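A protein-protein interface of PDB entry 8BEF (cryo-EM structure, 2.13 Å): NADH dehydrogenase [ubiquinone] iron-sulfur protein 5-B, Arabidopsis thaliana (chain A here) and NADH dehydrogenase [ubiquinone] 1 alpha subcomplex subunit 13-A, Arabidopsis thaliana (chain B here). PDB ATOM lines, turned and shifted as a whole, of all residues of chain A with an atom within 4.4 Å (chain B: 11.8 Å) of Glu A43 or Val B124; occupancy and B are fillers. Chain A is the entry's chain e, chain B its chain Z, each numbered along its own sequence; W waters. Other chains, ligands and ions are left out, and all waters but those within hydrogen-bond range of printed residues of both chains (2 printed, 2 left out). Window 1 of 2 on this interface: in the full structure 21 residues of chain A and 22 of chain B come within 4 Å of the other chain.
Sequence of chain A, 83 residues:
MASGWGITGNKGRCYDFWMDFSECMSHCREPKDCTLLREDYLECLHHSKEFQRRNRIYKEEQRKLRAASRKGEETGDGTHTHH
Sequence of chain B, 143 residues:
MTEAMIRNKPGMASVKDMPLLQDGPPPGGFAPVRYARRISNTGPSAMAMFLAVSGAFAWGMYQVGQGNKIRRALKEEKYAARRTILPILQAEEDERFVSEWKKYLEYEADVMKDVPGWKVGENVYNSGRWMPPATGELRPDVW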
ATOM      1  N   GLU A  39      -1.362 -38.166  17.220  1.00  0.00           N
ATOM      2  CA  GLU A  39      -1.870 -37.151  18.132  1.00  0.00           C
ATOM      3  C   GLU A  39      -3.314 -36.793  17.808  1.00  0.00           C
ATOM      4  O   GLU A  39      -4.063 -36.413  18.709  1.00  0.00           O
ATOM      5  CB  GLU A  39      -0.964 -35.916  18.124  1.00  0.00           C
ATOM      6  CG  GLU A  39      -1.024 -35.060  16.889  1.00  0.00           C
ATOM      7  CD  GLU A  39       0.212 -34.192  16.744  1.00  0.00           C
ATOM      8  OE1 GLU A  39       1.276 -34.591  17.256  1.00  0.00           O
ATOM      9  OE2 GLU A  39       0.120 -33.105  16.137  1.00  0.00           O
ATOM     10  N   ASP A  40      -3.740 -36.961  16.553  1.00  0.00           N
ATOM     11  CA  ASP A  40      -5.160 -36.822  16.243  1.00  0.00           C
ATOM     12  C   ASP A  40      -5.988 -37.899  16.941  1.00  0.00           C
ATOM     13  O   ASP A  40      -7.054 -37.611  17.501  1.00  0.00           O
ATOM     14  CB  ASP A  40      -5.377 -36.873  14.732  1.00  0.00           C
ATOM     15  CG  ASP A  40      -5.336 -35.496  14.093  1.00  0.00           C
ATOM     16  OD1 ASP A  40      -4.879 -34.545  14.761  1.00  0.00           O
ATOM     17  OD2 ASP A  40      -5.751 -35.367  12.925  1.00  0.00           O
ATOM     18  N   TYR A  41      -5.590 -39.166  16.861  1.00  0.00           N
ATOM     19  CA  TYR A  41      -6.246 -40.281  17.612  1.00  0.00           C
ATOM     20  C   TYR A  41      -6.316 -39.957  19.118  1.00  0.00           C
ATOM     21  O   TYR A  41      -7.392 -39.964  19.625  1.00  0.00           O
ATOM     22  CB  TYR A  41      -5.558 -41.614  17.291  1.00  0.00           C
ATOM     23  CG  TYR A  41      -6.031 -42.732  18.193  1.00  0.00           C
ATOM     24  CD1 TYR A  41      -7.310 -43.237  18.075  1.00  0.00           C
ATOM     25  CD2 TYR A  41      -5.229 -43.228  19.208  1.00  0.00           C
ATOM     26  CE1 TYR A  41      -7.769 -44.245  18.904  1.00  0.00           C
ATOM     27  CE2 TYR A  41      -5.665 -44.236  20.052  1.00  0.00           C
ATOM     28  CZ  TYR A  41      -6.946 -44.745  19.897  1.00  0.00           C
ATOM     29  OH  TYR A  41      -7.413 -45.733  20.701  1.00  0.00           O
ATOM     30  N   LEU A  42      -5.196 -39.571  19.721  1.00  0.00           N
ATOM     31  CA  LEU A  42      -5.209 -39.316  21.160  1.00  0.00           C
ATOM     32  C   LEU A  42      -6.044 -38.086  21.514  1.00  0.00           C
ATOM     33  O   LEU A  42      -6.684 -38.057  22.575  1.00  0.00           O
ATOM     34  CB  LEU A  42      -3.780 -39.183  21.681  1.00  0.00           C
ATOM     35  CG  LEU A  42      -2.926 -40.452  21.551  1.00  0.00           C
ATOM     36  CD1 LEU A  42      -1.524 -40.226  22.090  1.00  0.00           C
ATOM     37  CD2 LEU A  42      -3.578 -41.643  22.244  1.00  0.00           C
ATOM     38  N   GLU A  43      -6.064 -37.073  20.641  1.00  0.00           N
ATOM     39  CA  GLU A  43      -6.941 -35.924  20.837  1.00  0.00           C
ATOM     40  C   GLU A  43      -8.405 -36.334  20.790  1.00  0.00           C
ATOM     41  O   GLU A  43      -9.220 -35.838  21.573  1.00  0.00           O
ATOM     42  CB  GLU A  43      -6.650 -34.862  19.773  1.00  0.00           C
ATOM     43  CG  GLU A  43      -7.518 -33.605  19.840  1.00  0.00           C
ATOM     44  CD  GLU A  43      -7.412 -32.855  21.161  1.00  0.00           C
ATOM     45  OE1 GLU A  43      -6.348 -32.910  21.808  1.00  0.00           O
ATOM     46  OE2 GLU A  43      -8.396 -32.194  21.546  1.00  0.00           O
ATOM     47  N   CYS A  44      -8.761 -37.227  19.866  1.00  0.00           N
ATOM     48  CA  CYS A  44     -10.123 -37.750  19.859  1.00  0.00           C
ATOM     49  C   CYS A  44     -10.427 -38.486  21.158  1.00  0.00           C
ATOM     50  O   CYS A  44     -11.542 -38.395  21.685  1.00  0.00           O
ATOM     51  CB  CYS A  44     -10.341 -38.669  18.659  1.00  0.00           C
ATOM     52  SG  CYS A  44     -12.018 -39.332  18.528  1.00  0.00           S
ATOM     53  N   LEU A  45      -9.520 -39.173  21.778  1.00  0.00           N
ATOM     54  CA  LEU A  45      -9.816 -39.929  23.029  1.00  0.00           C
ATOM     55  C   LEU A  45     -10.007 -38.950  24.182  1.00  0.00           C
ATOM     56  O   LEU A  45     -10.933 -39.121  24.905  1.00  0.00           O
ATOM     57  CB  LEU A  45      -8.669 -40.836  23.451  1.00  0.00           C
ATOM     58  CG  LEU A  45      -8.300 -42.009  22.541  1.00  0.00           C
ATOM     59  CD1 LEU A  45      -7.228 -42.859  23.199  1.00  0.00           C
ATOM     60  CD2 LEU A  45      -9.492 -42.864  22.178  1.00  0.00           C
ATOM     61  N   HIS A  46      -9.117 -37.956  24.263  1.00  0.00           N
ATOM     62  CA  HIS A  46      -9.165 -37.169  25.491  1.00  0.00           C
ATOM     63  C   HIS A  46      -9.530 -35.696  25.325  1.00  0.00           C
ATOM     64  O   HIS A  46      -9.775 -35.033  26.339  1.00  0.00           O
ATOM     65  CB  HIS A  46      -7.824 -37.258  26.235  1.00  0.00           C
ATOM     66  CG  HIS A  46      -7.252 -38.640  26.290  1.00  0.00           C
ATOM     67  ND1 HIS A  46      -7.806 -39.646  27.050  1.00  0.00           N
ATOM     68  CD2 HIS A  46      -6.167 -39.180  25.685  1.00  0.00           C
ATOM     69  CE1 HIS A  46      -7.093 -40.748  26.908  1.00  0.00           C
ATOM     70  NE2 HIS A  46      -6.093 -40.493  26.085  1.00  0.00           N
ATOM     71  N   HIS A  47      -9.572 -35.164  24.102  1.00  0.00           N
ATOM     72  CA  HIS A  47      -9.921 -33.758  23.855  1.00  0.00           C
ATOM     73  C   HIS A  47      -9.035 -32.792  24.640  1.00  0.00           C
ATOM     74  O   HIS A  47      -9.494 -31.736  25.076  1.00  0.00           O
ATOM     75  CB  HIS A  47     -11.393 -33.471  24.174  1.00  0.00           C
ATOM     76  CG  HIS A  47     -12.344 -34.507  23.666  1.00  0.00           C
ATOM     77  ND1 HIS A  47     -12.560 -34.725  22.322  1.00  0.00           N
ATOM     78  CD2 HIS A  47     -13.150 -35.375  24.322  1.00  0.00           C
ATOM     79  CE1 HIS A  47     -13.454 -35.685  22.173  1.00  0.00           C
ATOM     80  NE2 HIS A  47     -13.827 -36.097  23.370  1.00  0.00           N
ATOM     81  N   SER A  48      -7.762 -33.138  24.828  1.00  0.00           N
ATOM     82  CA  SER A  48      -6.908 -32.344  25.703  1.00  0.00           C
ATOM     83  C   SER A  48      -6.647 -30.955  25.124  1.00  0.00           C
ATOM     84  O   SER A  48      -6.808 -29.945  25.818  1.00  0.00           O
ATOM     85  CB  SER A  48      -5.595 -33.082  25.963  1.00  0.00           C
ATOM     86  OG  SER A  48      -4.550 -32.179  26.271  1.00  0.00           O
ATOM     87  N   LYS A  49      -6.255 -30.882  23.851  1.00  0.00           N
ATOM     88  CA  LYS A  49      -5.926 -29.584  23.266  1.00  0.00           C
ATOM     89  C   LYS A  49      -7.169 -28.723  23.073  1.00  0.00           C
ATOM     90  O   LYS A  49      -7.122 -27.503  23.279  1.00  0.00           O
ATOM     91  CB  LYS A  49      -5.173 -29.768  21.949  1.00  0.00           C
ATOM     92  CG  LYS A  49      -3.793 -30.382  22.126  1.00  0.00           C
ATOM     93  CD  LYS A  49      -3.138 -30.769  20.805  1.00  0.00           C
ATOM     94  CE  LYS A  49      -4.119 -31.311  19.797  1.00  0.00           C
ATOM     95  NZ  LYS A  49      -4.344 -32.754  20.025  1.00  0.00           N
ATOM     96  N   GLU A  50      -8.287 -29.338  22.686  1.00  0.00           N
ATOM     97  CA  GLU A  50      -9.545 -28.608  22.557  1.00  0.00           C
ATOM     98  C   GLU A  50      -9.926 -27.932  23.868  1.00  0.00           C
ATOM     99  O   GLU A  50     -10.202 -26.723  23.908  1.00  0.00           O
ATOM    100  CB  GLU A  50     -10.650 -29.570  22.112  1.00  0.00           C
ATOM    101  CG  GLU A  50     -11.752 -28.946  21.274  1.00  0.00           C
ATOM    102  CD  GLU A  50     -12.996 -29.816  21.199  1.00  0.00           C
ATOM    103  OE1 GLU A  50     -12.915 -30.932  20.643  1.00  0.00           O
ATOM    104  OE2 GLU A  50     -14.062 -29.381  21.675  1.00  0.00           O
ATOM    105  N   TRP B 101     -22.680 -21.693  15.588  1.00  0.00           N
ATOM    106  CA  TRP B 101     -21.228 -21.701  15.474  1.00  0.00           C
ATOM    107  C   TRP B 101     -20.705 -20.360  14.978  1.00  0.00           C
ATOM    108  O   TRP B 101     -19.653 -19.898  15.431  1.00  0.00           O
ATOM    109  CB  TRP B 101     -20.777 -22.827  14.547  1.00  0.00           C
ATOM    110  CG  TRP B 101     -19.299 -22.999  14.542  1.00  0.00           C
ATOM    111  CD1 TRP B 101     -18.446 -22.758  13.506  1.00  0.00           C
ATOM    112  CD2 TRP B 101     -18.489 -23.436  15.636  1.00  0.00           C
ATOM    113  NE1 TRP B 101     -17.154 -23.024  13.885  1.00  0.00           N
ATOM    114  CE2 TRP B 101     -17.154 -23.443  15.189  1.00  0.00           C
ATOM    115  CE3 TRP B 101     -18.763 -23.826  16.951  1.00  0.00           C
ATOM    116  CZ2 TRP B 101     -16.099 -23.822  16.008  1.00  0.00           C
ATOM    117  CZ3 TRP B 101     -17.712 -24.206  17.761  1.00  0.00           C
ATOM    118  CH2 TRP B 101     -16.396 -24.199  17.287  1.00  0.00           C
ATOM    119  N   TYR B 104     -20.788 -18.092  17.971  1.00  0.00           N
ATOM    120  CA  TYR B 104     -19.701 -18.396  18.897  1.00  0.00           C
ATOM    121  C   TYR B 104     -18.356 -17.942  18.342  1.00  0.00           C
ATOM    122  O   TYR B 104     -17.477 -17.518  19.098  1.00  0.00           O
ATOM    123  CB  TYR B 104     -19.673 -19.892  19.215  1.00  0.00           C
ATOM    124  CG  TYR B 104     -18.434 -20.312  19.969  1.00  0.00           C
ATOM    125  CD1 TYR B 104     -18.328 -20.104  21.337  1.00  0.00           C
ATOM    126  CD2 TYR B 104     -17.365 -20.902  19.312  1.00  0.00           C
ATOM    127  CE1 TYR B 104     -17.196 -20.477  22.026  1.00  0.00           C
ATOM    128  CE2 TYR B 104     -16.230 -21.278  19.993  1.00  0.00           C
ATOM    129  CZ  TYR B 104     -16.150 -21.064  21.349  1.00  0.00           C
ATOM    130  OH  TYR B 104     -15.017 -21.439  22.030  1.00  0.00           O
ATOM    131  N   LEU B 105     -18.171 -18.036  17.026  1.00  0.00           N
ATOM    132  CA  LEU B 105     -16.928 -17.565  16.427  1.00  0.00           C
ATOM    133  C   LEU B 105     -16.785 -16.055  16.560  1.00  0.00           C
ATOM    134  O   LEU B 105     -15.689 -15.556  16.834  1.00  0.00           O
ATOM    135  CB  LEU B 105     -16.848 -17.994  14.964  1.00  0.00           C
ATOM    136  CG  LEU B 105     -15.886 -19.153  14.708  1.00  0.00           C
ATOM    137  CD1 LEU B 105     -16.093 -20.250  15.738  1.00  0.00           C
ATOM    138  CD2 LEU B 105     -16.069 -19.698  13.306  1.00  0.00           C
ATOM    139  N   GLU B 108     -15.756 -15.465  20.145  1.00  0.00           N
ATOM    140  CA  GLU B 108     -14.351 -15.779  20.385  1.00  0.00           C
ATOM    141  C   GLU B 108     -13.435 -14.740  19.748  1.00  0.00           C
ATOM    142  O   GLU B 108     -12.391 -14.392  20.314  1.00  0.00           O
ATOM    143  CB  GLU B 108     -14.031 -17.178  19.859  1.00  0.00           C
ATOM    144  CG  GLU B 108     -12.550 -17.491  19.746  1.00  0.00           C
ATOM    145  CD  GLU B 108     -12.287 -18.939  19.377  1.00  0.00           C
ATOM    146  OE1 GLU B 108     -11.363 -19.195  18.580  1.00  0.00           O
ATOM    147  OE2 GLU B 108     -13.010 -19.821  19.882  1.00  0.00           O
ATOM    148  N   TRP B 118      -3.283 -15.759  18.267  1.00  0.00           N
ATOM    149  CA  TRP B 118      -4.515 -16.525  18.214  1.00  0.00           C
ATOM    150  C   TRP B 118      -4.975 -16.728  16.772  1.00  0.00           C
ATOM    151  O   TRP B 118      -4.596 -15.995  15.855  1.00  0.00           O
ATOM    152  CB  TRP B 118      -5.615 -15.833  19.020  1.00  0.00           C
ATOM    153  CG  TRP B 118      -6.627 -16.782  19.565  1.00  0.00           C
ATOM    154  CD1 TRP B 118      -7.932 -16.894  19.188  1.00  0.00           C
ATOM    155  CD2 TRP B 118      -6.415 -17.772  20.579  1.00  0.00           C
ATOM    156  NE1 TRP B 118      -8.550 -17.889  19.907  1.00  0.00           N
ATOM    157  CE2 TRP B 118      -7.642 -18.442  20.770  1.00  0.00           C
ATOM    158  CE3 TRP B 118      -5.312 -18.154  21.345  1.00  0.00           C
ATOM    159  CZ2 TRP B 118      -7.792 -19.473  21.695  1.00  0.00           C
ATOM    160  CZ3 TRP B 118      -5.464 -19.178  22.263  1.00  0.00           C
ATOM    161  CH2 TRP B 118      -6.695 -19.824  22.430  1.00  0.00           C
ATOM    162  N   LYS B 119      -5.794 -17.761  16.585  1.00  0.00           N
ATOM    163  CA  LYS B 119      -6.482 -18.023  15.326  1.00  0.00           C
ATOM    164  C   LYS B 119      -7.897 -18.456  15.661  1.00  0.00           C
ATOM    165  O   LYS B 119      -8.093 -19.496  16.296  1.00  0.00           O
ATOM    166  CB  LYS B 119      -5.771 -19.101  14.504  1.00  0.00           C
ATOM    167  CG  LYS B 119      -4.516 -18.631  13.801  1.00  0.00           C
ATOM    168  CD  LYS B 119      -3.571 -19.788  13.532  1.00  0.00           C
ATOM    169  CE  LYS B 119      -2.400 -19.350  12.670  1.00  0.00           C
ATOM    170  NZ  LYS B 119      -2.830 -19.055  11.276  1.00  0.00           N
ATOM    171  N   VAL B 120      -8.880 -17.667  15.231  1.00  0.00           N
ATOM    172  CA  VAL B 120     -10.255 -17.881  15.663  1.00  0.00           C
ATOM    173  C   VAL B 120     -10.801 -19.153  15.031  1.00  0.00           C
ATOM    174  O   VAL B 120     -10.724 -19.343  13.810  1.00  0.00           O
ATOM    175  CB  VAL B 120     -11.119 -16.659  15.316  1.00  0.00           C
ATOM    176  CG1 VAL B 120     -12.597 -16.996  15.435  1.00  0.00           C
ATOM    177  CG2 VAL B 120     -10.757 -15.492  16.221  1.00  0.00           C
ATOM    178  N   GLY B 121     -11.352 -20.031  15.862  1.00  0.00           N
ATOM    179  CA  GLY B 121     -11.892 -21.294  15.382  1.00  0.00           C
ATOM    180  C   GLY B 121     -10.859 -22.211  14.763  1.00  0.00           C
ATOM    181  O   GLY B 121     -11.129 -22.842  13.735  1.00  0.00           O
ATOM    182  N   GLU B 122      -9.676 -22.298  15.365  1.00  0.00           N
ATOM    183  CA  GLU B 122      -8.638 -23.174  14.840  1.00  0.00           C
ATOM    184  C   GLU B 122      -9.004 -24.633  15.093  1.00  0.00           C
ATOM    185  O   GLU B 122      -9.392 -25.004  16.203  1.00  0.00           O
ATOM    186  CB  GLU B 122      -7.290 -22.838  15.480  1.00  0.00           C
ATOM    187  CG  GLU B 122      -6.218 -23.884  15.258  1.00  0.00           C
ATOM    188  CD  GLU B 122      -4.811 -23.317  15.330  1.00  0.00           C
ATOM    189  OE1 GLU B 122      -4.110 -23.340  14.298  1.00  0.00           O
ATOM    190  OE2 GLU B 122      -4.405 -22.856  16.418  1.00  0.00           O
ATOM    191  N   ASN B 123      -8.884 -25.461  14.057  1.00  0.00           N
ATOM    192  CA  ASN B 123      -9.120 -26.892  14.196  1.00  0.00           C
ATOM    193  C   ASN B 123      -7.939 -27.538  14.913  1.00  0.00           C
ATOM    194  O   ASN B 123      -6.796 -27.431  14.459  1.00  0.00           O
ATOM    195  CB  ASN B 123      -9.329 -27.527  12.824  1.00  0.00           C
ATOM    196  CG  ASN B 123      -9.948 -28.912  12.900  1.00  0.00           C
ATOM    197  OD1 ASN B 123      -9.887 -29.583  13.930  1.00  0.00           O
ATOM    198  ND2 ASN B 123     -10.543 -29.348  11.800  1.00  0.00           N
ATOM    199  N   VAL B 124      -8.209 -28.211  16.033  1.00  0.00           N
ATOM    200  CA  VAL B 124      -7.121 -28.836  16.778  1.00  0.00           C
ATOM    201  C   VAL B 124      -6.670 -30.148  16.146  1.00  0.00           C
ATOM    202  O   VAL B 124      -5.588 -30.643  16.481  1.00  0.00           O
ATOM    203  CB  VAL B 124      -7.505 -29.068  18.250  1.00  0.00           C
ATOM    204  CG1 VAL B 124      -7.721 -27.736  18.964  1.00  0.00           C
ATOM    205  CG2 VAL B 124      -8.731 -29.961  18.358  1.00  0.00           C
ATOM    206  N   TYR B 125      -7.463 -30.725  15.247  1.00  0.00           N
ATOM    207  CA  TYR B 125      -7.071 -31.947  14.559  1.00  0.00           C
ATOM    208  C   TYR B 125      -6.202 -31.613  13.354  1.00  0.00           C
ATOM    209  O   TYR B 125      -6.550 -30.746  12.547  1.00  0.00           O
ATOM    210  CB  TYR B 125      -8.309 -32.733  14.129  1.00  0.00           C
ATOM    211  CG  TYR B 125      -9.075 -33.312  15.296  1.00  0.00           C
ATOM    212  CD1 TYR B 125      -8.586 -34.410  15.990  1.00  0.00           C
ATOM    213  CD2 TYR B 125     -10.273 -32.748  15.717  1.00  0.00           C
ATOM    214  CE1 TYR B 125      -9.269 -34.939  17.063  1.00  0.00           C
ATOM    215  CE2 TYR B 125     -10.967 -33.274  16.791  1.00  0.00           C
ATOM    216  CZ  TYR B 125     -10.457 -34.371  17.460  1.00  0.00           C
ATOM    217  OH  TYR B 125     -11.134 -34.901  18.528  1.00  0.00           O
ATOM    218  N   ASN B 126      -5.061 -32.299  13.241  1.00  0.00           N
ATOM    219  CA  ASN B 126      -4.154 -32.058  12.122  1.00  0.00           C
ATOM    220  C   ASN B 126      -4.801 -32.422  10.793  1.00  0.00           C
ATOM    221  O   ASN B 126      -4.641 -31.704   9.800  1.00  0.00           O
ATOM    222  CB  ASN B 126      -2.861 -32.843  12.316  1.00  0.00           C
ATOM    223  CG  ASN B 126      -2.161 -32.493  13.606  1.00  0.00           C
ATOM    224  OD1 ASN B 126      -2.052 -33.318  14.506  1.00  0.00           O
ATOM    225  ND2 ASN B 126      -1.689 -31.261  13.704  1.00  0.00           N
ATOM    226  N   SER B 127      -5.538 -33.533  10.755  1.00  0.00           N
ATOM    227  CA  SER B 127      -6.201 -33.941   9.525  1.00  0.00           C
ATOM    228  C   SER B 127      -7.204 -32.906   9.038  1.00  0.00           C
ATOM    229  O   SER B 127      -7.563 -32.913   7.857  1.00  0.00           O
ATOM    230  CB  SER B 127      -6.901 -35.285   9.727  1.00  0.00           C
ATOM    231  OG  SER B 127      -8.227 -35.102  10.189  1.00  0.00           O
ATOM    232  N   GLY B 128      -7.665 -32.019   9.919  1.00  0.00           N
ATOM    233  CA  GLY B 128      -8.632 -31.009   9.556  1.00  0.00           C
ATOM    234  C   GLY B 128     -10.036 -31.521   9.343  1.00  0.00           C
ATOM    235  O   GLY B 128     -10.925 -30.723   9.029  1.00  0.00           O
ATOM    236  N   ARG B 129     -10.270 -32.817   9.507  1.00  0.00           N
ATOM    237  CA  ARG B 129     -11.615 -33.345   9.348  1.00  0.00           C
ATOM    238  C   ARG B 129     -12.511 -32.841  10.473  1.00  0.00           C
ATOM    239  O   ARG B 129     -12.069 -32.626  11.606  1.00  0.00           O
ATOM    240  CB  ARG B 129     -11.581 -34.874   9.288  1.00  0.00           C
ATOM    241  CG  ARG B 129     -12.646 -35.593  10.084  1.00  0.00           C
ATOM    242  CD  ARG B 129     -12.539 -37.093   9.861  1.00  0.00           C
ATOM    243  NE  ARG B 129     -11.403 -37.712  10.533  1.00  0.00           N
ATOM    244  CZ  ARG B 129     -11.002 -38.959  10.314  1.00  0.00           C
ATOM    245  NH1 ARG B 129     -11.617 -39.739   9.442  1.00  0.00           N
ATOM    246  NH2 ARG B 129      -9.967 -39.438  10.996  1.00  0.00           N
ATOM    247  N   TRP B 130     -13.775 -32.618  10.139  1.00  0.00           N
ATOM    248  CA  TRP B 130     -14.690 -31.945  11.047  1.00  0.00           C
ATOM    249  C   TRP B 130     -15.163 -32.895  12.139  1.00  0.00           C
ATOM    250  O   TRP B 130     -15.559 -34.030  11.862  1.00  0.00           O
ATOM    251  CB  TRP B 130     -15.885 -31.389  10.278  1.00  0.00           C
ATOM    252  CG  TRP B 130     -16.768 -30.554  11.129  1.00  0.00           C
ATOM    253  CD1 TRP B 130     -16.616 -29.230  11.413  1.00  0.00           C
ATOM    254  CD2 TRP B 130     -17.938 -30.985  11.829  1.00  0.00           C
ATOM    255  NE1 TRP B 130     -17.624 -28.808  12.243  1.00  0.00           N
ATOM    256  CE2 TRP B 130     -18.451 -29.866  12.511  1.00  0.00           C
ATOM    257  CE3 TRP B 130     -18.607 -32.207  11.938  1.00  0.00           C
ATOM    258  CZ2 TRP B 130     -19.600 -29.933  13.294  1.00  0.00           C
ATOM    259  CZ3 TRP B 130     -19.746 -32.271  12.714  1.00  0.00           C
ATOM    260  CH2 TRP B 130     -20.230 -31.142  13.384  1.00  0.00           C
ATOM    261  N   MET B 131     -15.124 -32.421  13.379  1.00  0.00           N
ATOM    262  CA  MET B 131     -15.690 -33.114  14.522  1.00  0.00           C
ATOM    263  C   MET B 131     -16.589 -32.155  15.286  1.00  0.00           C
ATOM    264  O   MET B 131     -16.306 -30.955  15.354  1.00  0.00           O
ATOM    265  CB  MET B 131     -14.594 -33.648  15.459  1.00  0.00           C
ATOM    266  CG  MET B 131     -13.645 -34.652  14.811  1.00  0.00           C
ATOM    267  SD  MET B 131     -14.358 -36.290  14.566  1.00  0.00           S
ATOM    268  CE  MET B 131     -14.827 -36.725  16.238  1.00  0.00           C
ATOM    269  N   PRO B 132     -17.682 -32.651  15.862  1.00  0.00           N
ATOM    270  CA  PRO B 132     -18.520 -31.787  16.687  1.00  0.00           C
ATOM    271  C   PRO B 132     -17.753 -31.315  17.904  1.00  0.00           C
ATOM    272  O   PRO B 132     -16.819 -31.993  18.374  1.00  0.00           O
ATOM    273  CB  PRO B 132     -19.697 -32.696  17.079  1.00  0.00           C
ATOM    274  CG  PRO B 132     -19.576 -33.930  16.271  1.00  0.00           C
ATOM    275  CD  PRO B 132     -18.181 -34.033  15.774  1.00  0.00           C
ATOM    276  N   PRO B 133     -18.098 -30.147  18.443  1.00  0.00           N
ATOM    277  CA  PRO B 133     -17.392 -29.659  19.636  1.00  0.00           C
ATOM    278  C   PRO B 133     -17.596 -30.601  20.815  1.00  0.00           C
ATOM    279  O   PRO B 133     -18.713 -31.038  21.100  1.00  0.00           O
ATOM    280  CB  PRO B 133     -18.018 -28.282  19.890  1.00  0.00           C
ATOM    281  CG  PRO B 133     -18.831 -27.965  18.672  1.00  0.00           C
ATOM    282  CD  PRO B 133     -19.214 -29.269  18.061  1.00  0.00           C
ATOM    283  N   ALA B 134     -16.498 -30.919  21.493  1.00  0.00           N
ATOM    284  CA  ALA B 134     -16.568 -31.771  22.669  1.00  0.00           C
ATOM    285  C   ALA B 134     -17.243 -31.023  23.813  1.00  0.00           C
ATOM    286  O   ALA B 134     -17.111 -29.805  23.953  1.00  0.00           O
ATOM    287  CB  ALA B 134     -15.169 -32.233  23.076  1.00  0.00           C
ATOM    288  N   THR B 135     -17.976 -31.767  24.640  1.00  0.00           N
ATOM    289  CA  THR B 135     -18.855 -31.156  25.625  1.00  0.00           C
ATOM    290  C   THR B 135     -18.374 -31.272  27.063  1.00  0.00           C
ATOM    291  O   THR B 135     -18.805 -30.477  27.901  1.00  0.00           O
ATOM    292  CB  THR B 135     -20.260 -31.763  25.526  1.00  0.00           C
ATOM    293  OG1 THR B 135     -20.307 -32.988  26.266  1.00  0.00           O
ATOM    294  CG2 THR B 135     -20.608 -32.040  24.077  1.00  0.00           C
ATOM    295  N   GLY B 136     -17.519 -32.222  27.352  1.00  0.00           N
ATOM    296  CA  GLY B 136     -17.008 -32.376  28.733  1.00  0.00           C
ATOM    297  C   GLY B 136     -18.020 -32.999  29.688  1.00  0.00           C
ATOM    298  O   GLY B 136     -17.863 -32.848  30.885  1.00  0.00           O
HETATM  299  O   HOH W   1     -10.908 -32.797  20.780  1.00  0.00           O
HETATM  300  O   HOH W   2     -14.221 -32.385  18.524  1.00  0.00           O
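Printed residues of chain A that touch a printed residue of chain B: Glu A39, Asp A40, Glu A43, Cys A44, His A47, Lys A49 and Glu A50. Hydrophobic or aromatic side chains of chain A that line the printed part of chain B: His A47. Of the 23 printed residues of chain B, 6 touch a printed residue of chain A.
Water W2 bridges O of Pro B132 and OE1 of Glu A50. Water W1 lies within hydrogen-bond range of the side-chain carboxylate of Glu A43, the side-chain carboxylate of Glu A50, a ring nitrogen (ND1) of His A47 and the side-chain hydroxyl of Tyr B125.
Among the printed residues, merely in contact across the chains: Asp A40 with Tyr B125 (3.4 Å), Glu A43 with Val B124 (3.9 Å), Glu A43 with Tyr B125 (3.5 Å), Cys A44 with Tyr B125 (3.3 Å), His A47 with Ala B134 (3.7 Å), Lys A49 with Val B124 (3.7 Å) and Glu A50 with Pro B133 (3.8 Å).
N of Asn B126 lies within hydrogen-bond range of OD1 of Asp A40 (2.7 Å). The backbone NH of Ala B134 sits at hydrogen-bond distance from the side-chain carboxylate of Glu A50. The backbone NH of Ser B127 is in hydrogen-bond range of the side-chain carboxylate of Asp A40 (2.8 Å). The side-chain amide oxygen (OD1) of Asn B126 sits close to the side-chain carboxylate (OE2) of Glu A39, at 2.7 Å.
The side-chain hydroxyl (OG) of Ser B127 sits close to the backbone NH (N) of Arg B129 (3.1 Å). OE1 of Glu A43 sits at hydrogen-bond distance from N of Ser A48, at 3.3 Å. The side-chain amino group (NZ) of Lys A49 is in salt-bridge range of the side-chain carboxylate (OE1) of Glu A43 (2.7 Å). N of Glu A50 lies within hydrogen-bond range of OE2 of Glu A43, at 3.1 Å. N of Tyr B125 is in hydrogen-bond range of OD1 of Asn B123.
Glu A43 touches two residues of chain B. Of chain A, only Glu A43 (3.9 Å) and Lys A49 (3.7 Å) come within 4 Å of Val B124. Of chain B, only Tyr B125, Asn B126 and Ser B127 come within 4 Å of Asp A40. No residue of chain B comes within 4 Å of Leu A42. Of chain B, only Tyr B125 (3.3 Å) comes within 4 Å of Cys A44. Of chain B, only Ala B134 comes within 4 Å of His A47. Of chain B, only Val B124 comes within 4 Å of Lys A49. Of the printed residues of chain A, Ala B134 touches His A47 (3.7 Å) and Glu A50 (2.9 Å). Of the printed residues of chain A, Tyr B125 touches Asp A40, Glu A43 and Cys A44. Printed residues of chain A within 4 Å of Asn B126: Glu A39 (2.7 Å) and Asp A40 (2.7 Å). Tyr A41 touches none of the printed residues of chain B. The nearest residue of chain B that does not touch Glu A43 is Ala B134 (6.9 Å). The nearest residue of chain A that does not touch Val B124 is Glu A50 (4.1 Å).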
